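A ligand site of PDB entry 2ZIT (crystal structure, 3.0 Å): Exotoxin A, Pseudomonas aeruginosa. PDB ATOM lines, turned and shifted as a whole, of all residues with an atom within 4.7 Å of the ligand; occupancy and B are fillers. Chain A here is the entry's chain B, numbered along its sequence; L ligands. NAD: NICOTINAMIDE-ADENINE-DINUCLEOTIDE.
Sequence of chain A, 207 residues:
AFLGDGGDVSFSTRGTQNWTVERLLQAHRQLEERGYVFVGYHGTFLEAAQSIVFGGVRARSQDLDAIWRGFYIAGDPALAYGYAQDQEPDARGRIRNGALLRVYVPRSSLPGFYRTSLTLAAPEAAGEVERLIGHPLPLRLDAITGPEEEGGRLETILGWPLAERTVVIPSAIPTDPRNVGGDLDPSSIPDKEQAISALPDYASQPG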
ATOM      1  N   TYR A  41      31.640 -12.590  12.083  1.00  0.00           N
ATOM      2  CA  TYR A  41      32.528 -13.032  11.019  1.00  0.00           C
ATOM      3  C   TYR A  41      31.752 -13.491   9.788  1.00  0.00           C
ATOM      4  O   TYR A  41      30.582 -13.847   9.874  1.00  0.00           O
ATOM      5  CB  TYR A  41      33.384 -14.198  11.509  1.00  0.00           C
ATOM      6  CG  TYR A  41      34.369 -13.857  12.595  1.00  0.00           C
ATOM      7  CD1 TYR A  41      35.675 -13.480  12.294  1.00  0.00           C
ATOM      8  CD2 TYR A  41      33.999 -13.915  13.931  1.00  0.00           C
ATOM      9  CE1 TYR A  41      36.574 -13.178  13.298  1.00  0.00           C
ATOM     10  CE2 TYR A  41      34.887 -13.612  14.936  1.00  0.00           C
ATOM     11  CZ  TYR A  41      36.180 -13.241  14.615  1.00  0.00           C
ATOM     12  OH  TYR A  41      37.077 -12.939  15.605  1.00  0.00           O
ATOM     13  N   HIS A  42      32.437 -13.498   8.656  1.00  0.00           N
ATOM     14  CA  HIS A  42      31.847 -13.991   7.407  1.00  0.00           C
ATOM     15  C   HIS A  42      32.898 -14.742   6.600  1.00  0.00           C
ATOM     16  O   HIS A  42      33.813 -14.131   6.039  1.00  0.00           O
ATOM     17  CB  HIS A  42      31.264 -12.835   6.590  1.00  0.00           C
ATOM     18  CG  HIS A  42      30.781 -13.245   5.233  1.00  0.00           C
ATOM     19  ND1 HIS A  42      29.467 -13.602   4.987  1.00  0.00           N
ATOM     20  CD2 HIS A  42      31.424 -13.348   4.053  1.00  0.00           C
ATOM     21  CE1 HIS A  42      29.328 -13.903   3.711  1.00  0.00           C
ATOM     22  NE2 HIS A  42      30.501 -13.764   3.120  1.00  0.00           N
ATOM     23  N   GLY A  43      32.784 -16.063   6.551  1.00  0.00           N
ATOM     24  CA  GLY A  43      33.714 -16.896   5.810  1.00  0.00           C
ATOM     25  C   GLY A  43      33.310 -17.039   4.350  1.00  0.00           C
ATOM     26  O   GLY A  43      32.128 -17.193   4.038  1.00  0.00           O
ATOM     27  N   THR A  44      34.304 -16.993   3.461  1.00  0.00           N
ATOM     28  CA  THR A  44      34.040 -17.065   2.033  1.00  0.00           C
ATOM     29  C   THR A  44      35.316 -17.303   1.219  1.00  0.00           C
ATOM     30  O   THR A  44      36.413 -17.356   1.782  1.00  0.00           O
ATOM     31  CB  THR A  44      33.353 -15.794   1.514  1.00  0.00           C
ATOM     32  OG1 THR A  44      33.146 -15.897   0.102  1.00  0.00           O
ATOM     33  CG2 THR A  44      34.209 -14.569   1.810  1.00  0.00           C
ATOM     34  N   PHE A  45      35.172 -17.447  -0.091  1.00  0.00           N
ATOM     35  CA  PHE A  45      36.312 -17.671  -0.970  1.00  0.00           C
ATOM     36  C   PHE A  45      37.050 -16.392  -1.347  1.00  0.00           C
ATOM     37  O   PHE A  45      36.495 -15.295  -1.247  1.00  0.00           O
ATOM     38  CB  PHE A  45      35.886 -18.438  -2.226  1.00  0.00           C
ATOM     39  CG  PHE A  45      34.819 -17.756  -3.030  1.00  0.00           C
ATOM     40  CD1 PHE A  45      33.501 -17.763  -2.600  1.00  0.00           C
ATOM     41  CD2 PHE A  45      35.125 -17.117  -4.226  1.00  0.00           C
ATOM     42  CE1 PHE A  45      32.510 -17.142  -3.347  1.00  0.00           C
ATOM     43  CE2 PHE A  45      34.135 -16.496  -4.972  1.00  0.00           C
ATOM     44  CZ  PHE A  45      32.828 -16.504  -4.529  1.00  0.00           C
ATOM     45  N   ALA A  48      35.606 -13.541  -3.485  1.00  0.00           N
ATOM     46  CA  ALA A  48      34.476 -12.948  -2.786  1.00  0.00           C
ATOM     47  C   ALA A  48      34.965 -11.952  -1.738  1.00  0.00           C
ATOM     48  O   ALA A  48      34.482 -10.821  -1.682  1.00  0.00           O
ATOM     49  CB  ALA A  48      33.617 -14.017  -2.148  1.00  0.00           C
ATOM     50  N   SER A  51      36.075  -8.787  -3.302  1.00  0.00           N
ATOM     51  CA  SER A  51      34.927  -7.981  -3.705  1.00  0.00           C
ATOM     52  C   SER A  51      34.284  -7.273  -2.520  1.00  0.00           C
ATOM     53  O   SER A  51      33.861  -6.125  -2.620  1.00  0.00           O
ATOM     54  CB  SER A  51      33.892  -8.860  -4.401  1.00  0.00           C
ATOM     55  OG  SER A  51      32.739  -8.114  -4.737  1.00  0.00           O
ATOM     56  N   ILE A  52      34.193  -7.976  -1.394  1.00  0.00           N
ATOM     57  CA  ILE A  52      33.538  -7.439  -0.215  1.00  0.00           C
ATOM     58  C   ILE A  52      34.384  -6.350   0.443  1.00  0.00           C
ATOM     59  O   ILE A  52      33.897  -5.255   0.721  1.00  0.00           O
ATOM     60  CB  ILE A  52      33.240  -8.557   0.807  1.00  0.00           C
ATOM     61  CG1 ILE A  52      32.254  -9.553   0.209  1.00  0.00           C
ATOM     62  CG2 ILE A  52      32.699  -7.955   2.092  1.00  0.00           C
ATOM     63  CD1 ILE A  52      31.891 -10.687   1.131  1.00  0.00           C
ATOM     64  N   GLY A  56      32.751  -3.592  -1.266  1.00  0.00           N
ATOM     65  CA  GLY A  56      31.656  -3.494  -0.323  1.00  0.00           C
ATOM     66  C   GLY A  56      30.628  -4.596  -0.521  1.00  0.00           C
ATOM     67  O   GLY A  56      30.458  -5.105  -1.621  1.00  0.00           O
ATOM     68  N   VAL A  57      29.942  -4.952   0.554  1.00  0.00           N
ATOM     69  CA  VAL A  57      28.868  -5.937   0.499  1.00  0.00           C
ATOM     70  C   VAL A  57      27.726  -5.411  -0.370  1.00  0.00           C
ATOM     71  O   VAL A  57      27.149  -4.370  -0.066  1.00  0.00           O
ATOM     72  CB  VAL A  57      28.343  -6.266   1.905  1.00  0.00           C
ATOM     73  CG1 VAL A  57      27.078  -7.104   1.821  1.00  0.00           C
ATOM     74  CG2 VAL A  57      29.408  -6.975   2.739  1.00  0.00           C
ATOM     75  N   ARG A  58      27.389  -6.132  -1.430  1.00  0.00           N
ATOM     76  CA  ARG A  58      26.287  -5.759  -2.326  1.00  0.00           C
ATOM     77  C   ARG A  58      25.298  -6.901  -2.476  1.00  0.00           C
ATOM     78  O   ARG A  58      25.687  -8.069  -2.570  1.00  0.00           O
ATOM     79  CB  ARG A  58      26.820  -5.350  -3.700  1.00  0.00           C
ATOM     80  CG  ARG A  58      28.037  -4.426  -3.636  1.00  0.00           C
ATOM     81  CD  ARG A  58      28.517  -4.023  -5.018  1.00  0.00           C
ATOM     82  NE  ARG A  58      29.969  -3.822  -5.064  1.00  0.00           N
ATOM     83  CZ  ARG A  58      30.849  -4.805  -5.189  1.00  0.00           C
ATOM     84  NH1 ARG A  58      30.429  -6.059  -5.266  1.00  0.00           N
ATOM     85  NH2 ARG A  58      32.148  -4.549  -5.235  1.00  0.00           N
ATOM     86  N   ARG A  60      22.739  -9.708  -3.755  1.00  0.00           N
ATOM     87  CA  ARG A  60      22.778 -10.636  -4.868  1.00  0.00           C
ATOM     88  C   ARG A  60      21.796 -11.772  -4.635  1.00  0.00           C
ATOM     89  O   ARG A  60      21.355 -11.995  -3.506  1.00  0.00           O
ATOM     90  CB  ARG A  60      24.189 -11.205  -5.043  1.00  0.00           C
ATOM     91  CG  ARG A  60      24.837 -11.647  -3.742  1.00  0.00           C
ATOM     92  CD  ARG A  60      26.022 -12.583  -3.978  1.00  0.00           C
ATOM     93  NE  ARG A  60      27.029 -12.059  -4.894  1.00  0.00           N
ATOM     94  CZ  ARG A  60      27.419 -10.781  -4.971  1.00  0.00           C
ATOM     95  NH1 ARG A  60      26.908  -9.874  -4.164  1.00  0.00           N
ATOM     96  NH2 ARG A  60      28.346 -10.435  -5.850  1.00  0.00           N
ATOM     97  N   GLN A  62      20.406 -15.460  -4.017  1.00  0.00           N
ATOM     98  CA  GLN A  62      20.912 -16.544  -3.180  1.00  0.00           C
ATOM     99  C   GLN A  62      19.858 -17.643  -3.027  1.00  0.00           C
ATOM    100  O   GLN A  62      18.663 -17.373  -3.012  1.00  0.00           O
ATOM    101  CB  GLN A  62      21.346 -16.010  -1.824  1.00  0.00           C
ATOM    102  CG  GLN A  62      20.420 -14.957  -1.249  1.00  0.00           C
ATOM    103  CD  GLN A  62      21.027 -14.226  -0.068  1.00  0.00           C
ATOM    104  OE1 GLN A  62      20.587 -13.135   0.291  1.00  0.00           O
ATOM    105  NE2 GLN A  62      22.049 -14.825   0.539  1.00  0.00           N
ATOM    106  N   LEU A  64      17.568 -19.518  -1.418  1.00  0.00           N
ATOM    107  CA  LEU A  64      16.713 -19.622  -0.250  1.00  0.00           C
ATOM    108  C   LEU A  64      15.421 -18.853  -0.494  1.00  0.00           C
ATOM    109  O   LEU A  64      15.304 -18.127  -1.478  1.00  0.00           O
ATOM    110  CB  LEU A  64      17.419 -19.113   1.008  1.00  0.00           C
ATOM    111  CG  LEU A  64      18.187 -17.779   0.939  1.00  0.00           C
ATOM    112  CD1 LEU A  64      17.253 -16.607   0.677  1.00  0.00           C
ATOM    113  CD2 LEU A  64      18.965 -17.562   2.222  1.00  0.00           C
ATOM    114  N   GLY A  70      19.584 -11.891   2.538  1.00  0.00           N
ATOM    115  CA  GLY A  70      20.418 -10.974   3.297  1.00  0.00           C
ATOM    116  C   GLY A  70      21.838 -11.491   3.439  1.00  0.00           C
ATOM    117  O   GLY A  70      22.165 -12.570   2.950  1.00  0.00           O
ATOM    118  N   PHE A  71      22.679 -10.716   4.111  1.00  0.00           N
ATOM    119  CA  PHE A  71      24.067 -11.108   4.322  1.00  0.00           C
ATOM    120  C   PHE A  71      24.167 -11.959   5.583  1.00  0.00           C
ATOM    121  O   PHE A  71      23.617 -11.614   6.623  1.00  0.00           O
ATOM    122  CB  PHE A  71      24.950  -9.862   4.437  1.00  0.00           C
ATOM    123  CG  PHE A  71      26.419 -10.143   4.216  1.00  0.00           C
ATOM    124  CD1 PHE A  71      26.887 -10.486   2.956  1.00  0.00           C
ATOM    125  CD2 PHE A  71      27.317 -10.039   5.270  1.00  0.00           C
ATOM    126  CE1 PHE A  71      28.241 -10.737   2.753  1.00  0.00           C
ATOM    127  CE2 PHE A  71      28.671 -10.291   5.067  1.00  0.00           C
ATOM    128  CZ  PHE A  71      29.129 -10.632   3.809  1.00  0.00           C
ATOM    129  N   TYR A  72      24.872 -13.076   5.475  1.00  0.00           N
ATOM    130  CA  TYR A  72      24.968 -14.029   6.577  1.00  0.00           C
ATOM    131  C   TYR A  72      26.313 -13.981   7.288  1.00  0.00           C
ATOM    132  O   TYR A  72      27.361 -14.174   6.674  1.00  0.00           O
ATOM    133  CB  TYR A  72      24.662 -15.442   6.082  1.00  0.00           C
ATOM    134  CG  TYR A  72      23.188 -15.688   5.883  1.00  0.00           C
ATOM    135  CD1 TYR A  72      22.539 -15.273   4.732  1.00  0.00           C
ATOM    136  CD2 TYR A  72      22.434 -16.317   6.869  1.00  0.00           C
ATOM    137  CE1 TYR A  72      21.185 -15.489   4.555  1.00  0.00           C
ATOM    138  CE2 TYR A  72      21.079 -16.540   6.699  1.00  0.00           C
ATOM    139  CZ  TYR A  72      20.462 -16.117   5.545  1.00  0.00           C
ATOM    140  OH  TYR A  72      19.108 -16.340   5.375  1.00  0.00           O
ATOM    141  N   ILE A  73      26.265 -13.710   8.592  1.00  0.00           N
ATOM    142  CA  ILE A  73      27.474 -13.669   9.396  1.00  0.00           C
ATOM    143  C   ILE A  73      27.267 -14.479  10.673  1.00  0.00           C
ATOM    144  O   ILE A  73      26.148 -14.851  11.004  1.00  0.00           O
ATOM    145  CB  ILE A  73      27.857 -12.226   9.775  1.00  0.00           C
ATOM    146  CG1 ILE A  73      26.853 -11.659  10.783  1.00  0.00           C
ATOM    147  CG2 ILE A  73      27.947 -11.357   8.544  1.00  0.00           C
ATOM    148  CD1 ILE A  73      27.155 -10.235  11.208  1.00  0.00           C
ATOM    149  N   ALA A  74      28.359 -14.747  11.381  1.00  0.00           N
ATOM    150  CA  ALA A  74      28.287 -15.474  12.633  1.00  0.00           C
ATOM    151  C   ALA A  74      29.206 -14.864  13.687  1.00  0.00           C
ATOM    152  O   ALA A  74      30.330 -14.470  13.376  1.00  0.00           O
ATOM    153  CB  ALA A  74      28.641 -16.937  12.419  1.00  0.00           C
ATOM    154  N   LEU A  79      32.036 -21.158  13.148  1.00  0.00           N
ATOM    155  CA  LEU A  79      30.904 -21.398  12.251  1.00  0.00           C
ATOM    156  C   LEU A  79      31.176 -20.844  10.856  1.00  0.00           C
ATOM    157  O   LEU A  79      31.118 -21.581   9.867  1.00  0.00           O
ATOM    158  CB  LEU A  79      29.622 -20.785  12.824  1.00  0.00           C
ATOM    159  CG  LEU A  79      28.362 -20.963  11.974  1.00  0.00           C
ATOM    160  CD1 LEU A  79      28.181 -22.421  11.595  1.00  0.00           C
ATOM    161  CD2 LEU A  79      27.130 -20.437  12.701  1.00  0.00           C
ATOM    162  N   ALA A  80      31.475 -19.556  10.781  1.00  0.00           N
ATOM    163  CA  ALA A  80      31.758 -18.896   9.509  1.00  0.00           C
ATOM    164  C   ALA A  80      32.989 -19.513   8.835  1.00  0.00           C
ATOM    165  O   ALA A  80      33.152 -19.425   7.619  1.00  0.00           O
ATOM    166  CB  ALA A  80      31.960 -17.402   9.721  1.00  0.00           C
ATOM    167  N   TYR A  83      32.560 -21.922   5.916  1.00  0.00           N
ATOM    168  CA  TYR A  83      32.177 -21.419   4.605  1.00  0.00           C
ATOM    169  C   TYR A  83      33.344 -20.709   3.936  1.00  0.00           C
ATOM    170  O   TYR A  83      33.215 -20.204   2.819  1.00  0.00           O
ATOM    171  CB  TYR A  83      30.971 -20.480   4.723  1.00  0.00           C
ATOM    172  CG  TYR A  83      29.790 -21.108   5.412  1.00  0.00           C
ATOM    173  CD1 TYR A  83      28.826 -21.806   4.694  1.00  0.00           C
ATOM    174  CD2 TYR A  83      29.627 -20.999   6.791  1.00  0.00           C
ATOM    175  CE1 TYR A  83      27.741 -22.382   5.328  1.00  0.00           C
ATOM    176  CE2 TYR A  83      28.554 -21.570   7.431  1.00  0.00           C
ATOM    177  CZ  TYR A  83      27.609 -22.266   6.689  1.00  0.00           C
ATOM    178  OH  TYR A  83      26.535 -22.837   7.330  1.00  0.00           O
ATOM    179  N   GLU A 148      21.414 -21.441  13.880  1.00  0.00           N
ATOM    180  CA  GLU A 148      21.402 -21.809  12.458  1.00  0.00           C
ATOM    181  C   GLU A 148      20.579 -23.077  12.260  1.00  0.00           C
ATOM    182  O   GLU A 148      19.970 -23.275  11.208  1.00  0.00           O
ATOM    183  CB  GLU A 148      22.826 -22.006  11.933  1.00  0.00           C
ATOM    184  CG  GLU A 148      22.926 -22.948  10.743  1.00  0.00           C
ATOM    185  CD  GLU A 148      24.167 -22.692   9.898  1.00  0.00           C
ATOM    186  OE1 GLU A 148      24.481 -21.518   9.656  1.00  0.00           O
ATOM    187  OE2 GLU A 148      24.825 -23.675   9.477  1.00  0.00           O
ATOM    188  N   GLU A 155      23.726 -17.678  14.400  1.00  0.00           N
ATOM    189  CA  GLU A 155      24.054 -16.965  13.178  1.00  0.00           C
ATOM    190  C   GLU A 155      23.330 -15.614  13.172  1.00  0.00           C
ATOM    191  O   GLU A 155      22.390 -15.410  13.938  1.00  0.00           O
ATOM    192  CB  GLU A 155      23.641 -17.777  11.937  1.00  0.00           C
ATOM    193  CG  GLU A 155      22.140 -17.992  11.818  1.00  0.00           C
ATOM    194  CD  GLU A 155      21.752 -18.633  10.504  1.00  0.00           C
ATOM    195  OE1 GLU A 155      22.620 -18.773   9.614  1.00  0.00           O
ATOM    196  OE2 GLU A 155      20.560 -18.977  10.343  1.00  0.00           O
ATOM    197  N   TRP A 160      19.695  -6.809   3.572  1.00  0.00           N
ATOM    198  CA  TRP A 160      20.556  -6.193   2.554  1.00  0.00           C
ATOM    199  C   TRP A 160      20.745  -4.679   2.702  1.00  0.00           C
ATOM    200  O   TRP A 160      21.867  -4.186   2.600  1.00  0.00           O
ATOM    201  CB  TRP A 160      20.079  -6.543   1.144  1.00  0.00           C
ATOM    202  CG  TRP A 160      20.428  -7.944   0.758  1.00  0.00           C
ATOM    203  CD1 TRP A 160      19.562  -8.957   0.476  1.00  0.00           C
ATOM    204  CD2 TRP A 160      21.744  -8.494   0.620  1.00  0.00           C
ATOM    205  NE1 TRP A 160      20.252 -10.104   0.178  1.00  0.00           N
ATOM    206  CE2 TRP A 160      21.593  -9.848   0.255  1.00  0.00           C
ATOM    207  CE3 TRP A 160      23.026  -7.979   0.764  1.00  0.00           C
ATOM    208  CZ2 TRP A 160      22.684 -10.687   0.032  1.00  0.00           C
ATOM    209  CZ3 TRP A 160      24.109  -8.816   0.556  1.00  0.00           C
ATOM    210  CH2 TRP A 160      23.930 -10.158   0.186  1.00  0.00           C
HETATM  211  PA  NAD L   1      25.137 -16.819   0.031  1.00  0.00           P
HETATM  212  O1A NAD L   1      24.519 -17.504  -1.151  1.00  0.00           O
HETATM  213  O2A NAD L   1      24.252 -16.325   1.129  1.00  0.00           O
HETATM  214  O5B NAD L   1      25.998 -15.596  -0.563  1.00  0.00           O
HETATM  215  C5B NAD L   1      26.738 -15.889  -1.746  1.00  0.00           C
HETATM  216  C4B NAD L   1      28.212 -15.513  -1.673  1.00  0.00           C
HETATM  217  O4B NAD L   1      28.522 -14.355  -2.455  1.00  0.00           O
HETATM  218  C3B NAD L   1      28.763 -15.263  -0.268  1.00  0.00           C
HETATM  219  O3B NAD L   1      29.385 -16.444   0.262  1.00  0.00           O
HETATM  220  C2B NAD L   1      29.759 -14.128  -0.459  1.00  0.00           C
HETATM  221  O2B NAD L   1      31.059 -14.512  -0.018  1.00  0.00           O
HETATM  222  C1B NAD L   1      29.781 -13.874  -1.966  1.00  0.00           C
HETATM  223  N9A NAD L   1      30.067 -12.456  -2.315  1.00  0.00           N
HETATM  224  C8A NAD L   1      31.008 -12.047  -3.177  1.00  0.00           C
HETATM  225  N7A NAD L   1      30.972 -10.699  -3.247  1.00  0.00           N
HETATM  226  C5A NAD L   1      29.985 -10.269  -2.442  1.00  0.00           C
HETATM  227  C6A NAD L   1      29.502  -9.000  -2.129  1.00  0.00           C
HETATM  228  N6A NAD L   1      30.037  -7.897  -2.691  1.00  0.00           N
HETATM  229  N1A NAD L   1      28.473  -8.896  -1.257  1.00  0.00           N
HETATM  230  C2A NAD L   1      27.928  -9.990  -0.701  1.00  0.00           C
HETATM  231  N3A NAD L   1      28.380 -11.217  -0.992  1.00  0.00           N
HETATM  232  C4A NAD L   1      29.408 -11.392  -1.861  1.00  0.00           C
HETATM  233  O3  NAD L   1      26.270 -17.774   0.662  1.00  0.00           O
HETATM  234  PN  NAD L   1      26.783 -17.626   2.189  1.00  0.00           P
HETATM  235  O1N NAD L   1      26.215 -16.368   2.796  1.00  0.00           O
HETATM  236  O2N NAD L   1      28.265 -17.858   2.214  1.00  0.00           O
HETATM  237  O5D NAD L   1      26.054 -18.890   2.848  1.00  0.00           O
HETATM  238  C5D NAD L   1      24.654 -18.807   3.099  1.00  0.00           C
HETATM  239  C4D NAD L   1      24.203 -19.855   4.105  1.00  0.00           C
HETATM  240  O4D NAD L   1      25.283 -20.175   4.994  1.00  0.00           O
HETATM  241  C3D NAD L   1      23.084 -19.277   4.953  1.00  0.00           C
HETATM  242  O3D NAD L   1      21.822 -19.857   4.618  1.00  0.00           O
HETATM  243  C2D NAD L   1      23.456 -19.576   6.392  1.00  0.00           C
HETATM  244  O2D NAD L   1      22.556 -20.549   6.952  1.00  0.00           O
HETATM  245  C1D NAD L   1      24.862 -20.130   6.352  1.00  0.00           C
HETATM  246  N1N NAD L   1      25.771 -19.241   7.090  1.00  0.00           N
HETATM  247  C2N NAD L   1      26.836 -18.718   6.460  1.00  0.00           C
HETATM  248  C3N NAD L   1      27.727 -17.888   7.131  1.00  0.00           C
HETATM  249  C7N NAD L   1      28.905 -17.312   6.394  1.00  0.00           C
HETATM  250  O7N NAD L   1      29.814 -16.804   7.019  1.00  0.00           O
HETATM  251  N7N NAD L   1      28.923 -17.399   5.065  1.00  0.00           N
HETATM  252  C4N NAD L   1      27.521 -17.608   8.472  1.00  0.00           C
HETATM  253  C5N NAD L   1      26.419 -18.167   9.107  1.00  0.00           C
HETATM  254  C6N NAD L   1      25.565 -18.992   8.390  1.00  0.00           C
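O2D of the ligand lies close to OE1 of Glu 155.
N of Arg 58 is in hydrogen-bond range of N1A of the ligand, 3.0 Å away.
O2A of the ligand lies within hydrogen-bond range of NE2 of Gln 62.
An oxygen (O2B) of the ligand is in hydrogen-bond range of a ring nitrogen (NE2) of His 42, at 3.3 Å.
An oxygen (O2B) of the ligand sits at hydrogen-bond distance from the side-chain hydroxyl (OG1) of Thr 44, at 2.5 Å.
N6A of the ligand is in hydrogen-bond range of OG of Ser 51, 3.4 Å away.
The backbone NH (N) of Gly 43 is in hydrogen-bond range of an oxygen (O7N) of the ligand (3.1 Å).
N7N of the ligand lies within hydrogen-bond range of O of Gly 43 (3.4 Å).
The side-chain carboxylate (OE1) of Glu 148 sits close to an oxygen (O2D) of the ligand (3.5 Å).
N6A of the ligand lies within hydrogen-bond range of O of Gly 56 (3.0 Å).
The guanidinium group of Arg 60 sits close to a nitrogen (N1A) of the ligand (3.4 Å).
NE1 of Trp 160 sits at hydrogen-bond distance from OE1 of Gln 62 (3.1 Å).
The backbone carbonyl oxygen (O) of Tyr 72 sits at hydrogen-bond distance from a ring nitrogen (ND1) of His 42 (2.8 Å).
The backbone carbonyl oxygen (O) of Tyr 83 sits close to the backbone NH (N) of Thr 44, 3.5 Å away.
OG of Ser 51 lies within hydrogen-bond range of NH1 of Arg 58 (3.1 Å).
The side-chain carboxylate of Glu 148 sits at hydrogen-bond distance from the side-chain hydroxyl of Tyr 83, 2.9 Å away.
The guanidinium group of Arg 60 is in hydrogen-bond range of the backbone carbonyl oxygen of Arg 58.
The backbone NH of Gly 56 is in hydrogen-bond range of the backbone carbonyl oxygen of Ser 51 (3.1 Å).
N of Gly 70 is in hydrogen-bond range of OE1 of Gln 62 (2.8 Å).
Residues that only touch the ligand: Tyr 83, Ala 48, Tyr 72, Val 57, Ala 80, Phe 71, Ile 52 and Ile 73.
Along chain A the residues within 4 Å of the ligand span positions 42 to 155.
The nearest printed residue that does not touch the ligand is Trp 160 (4.1 Å).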
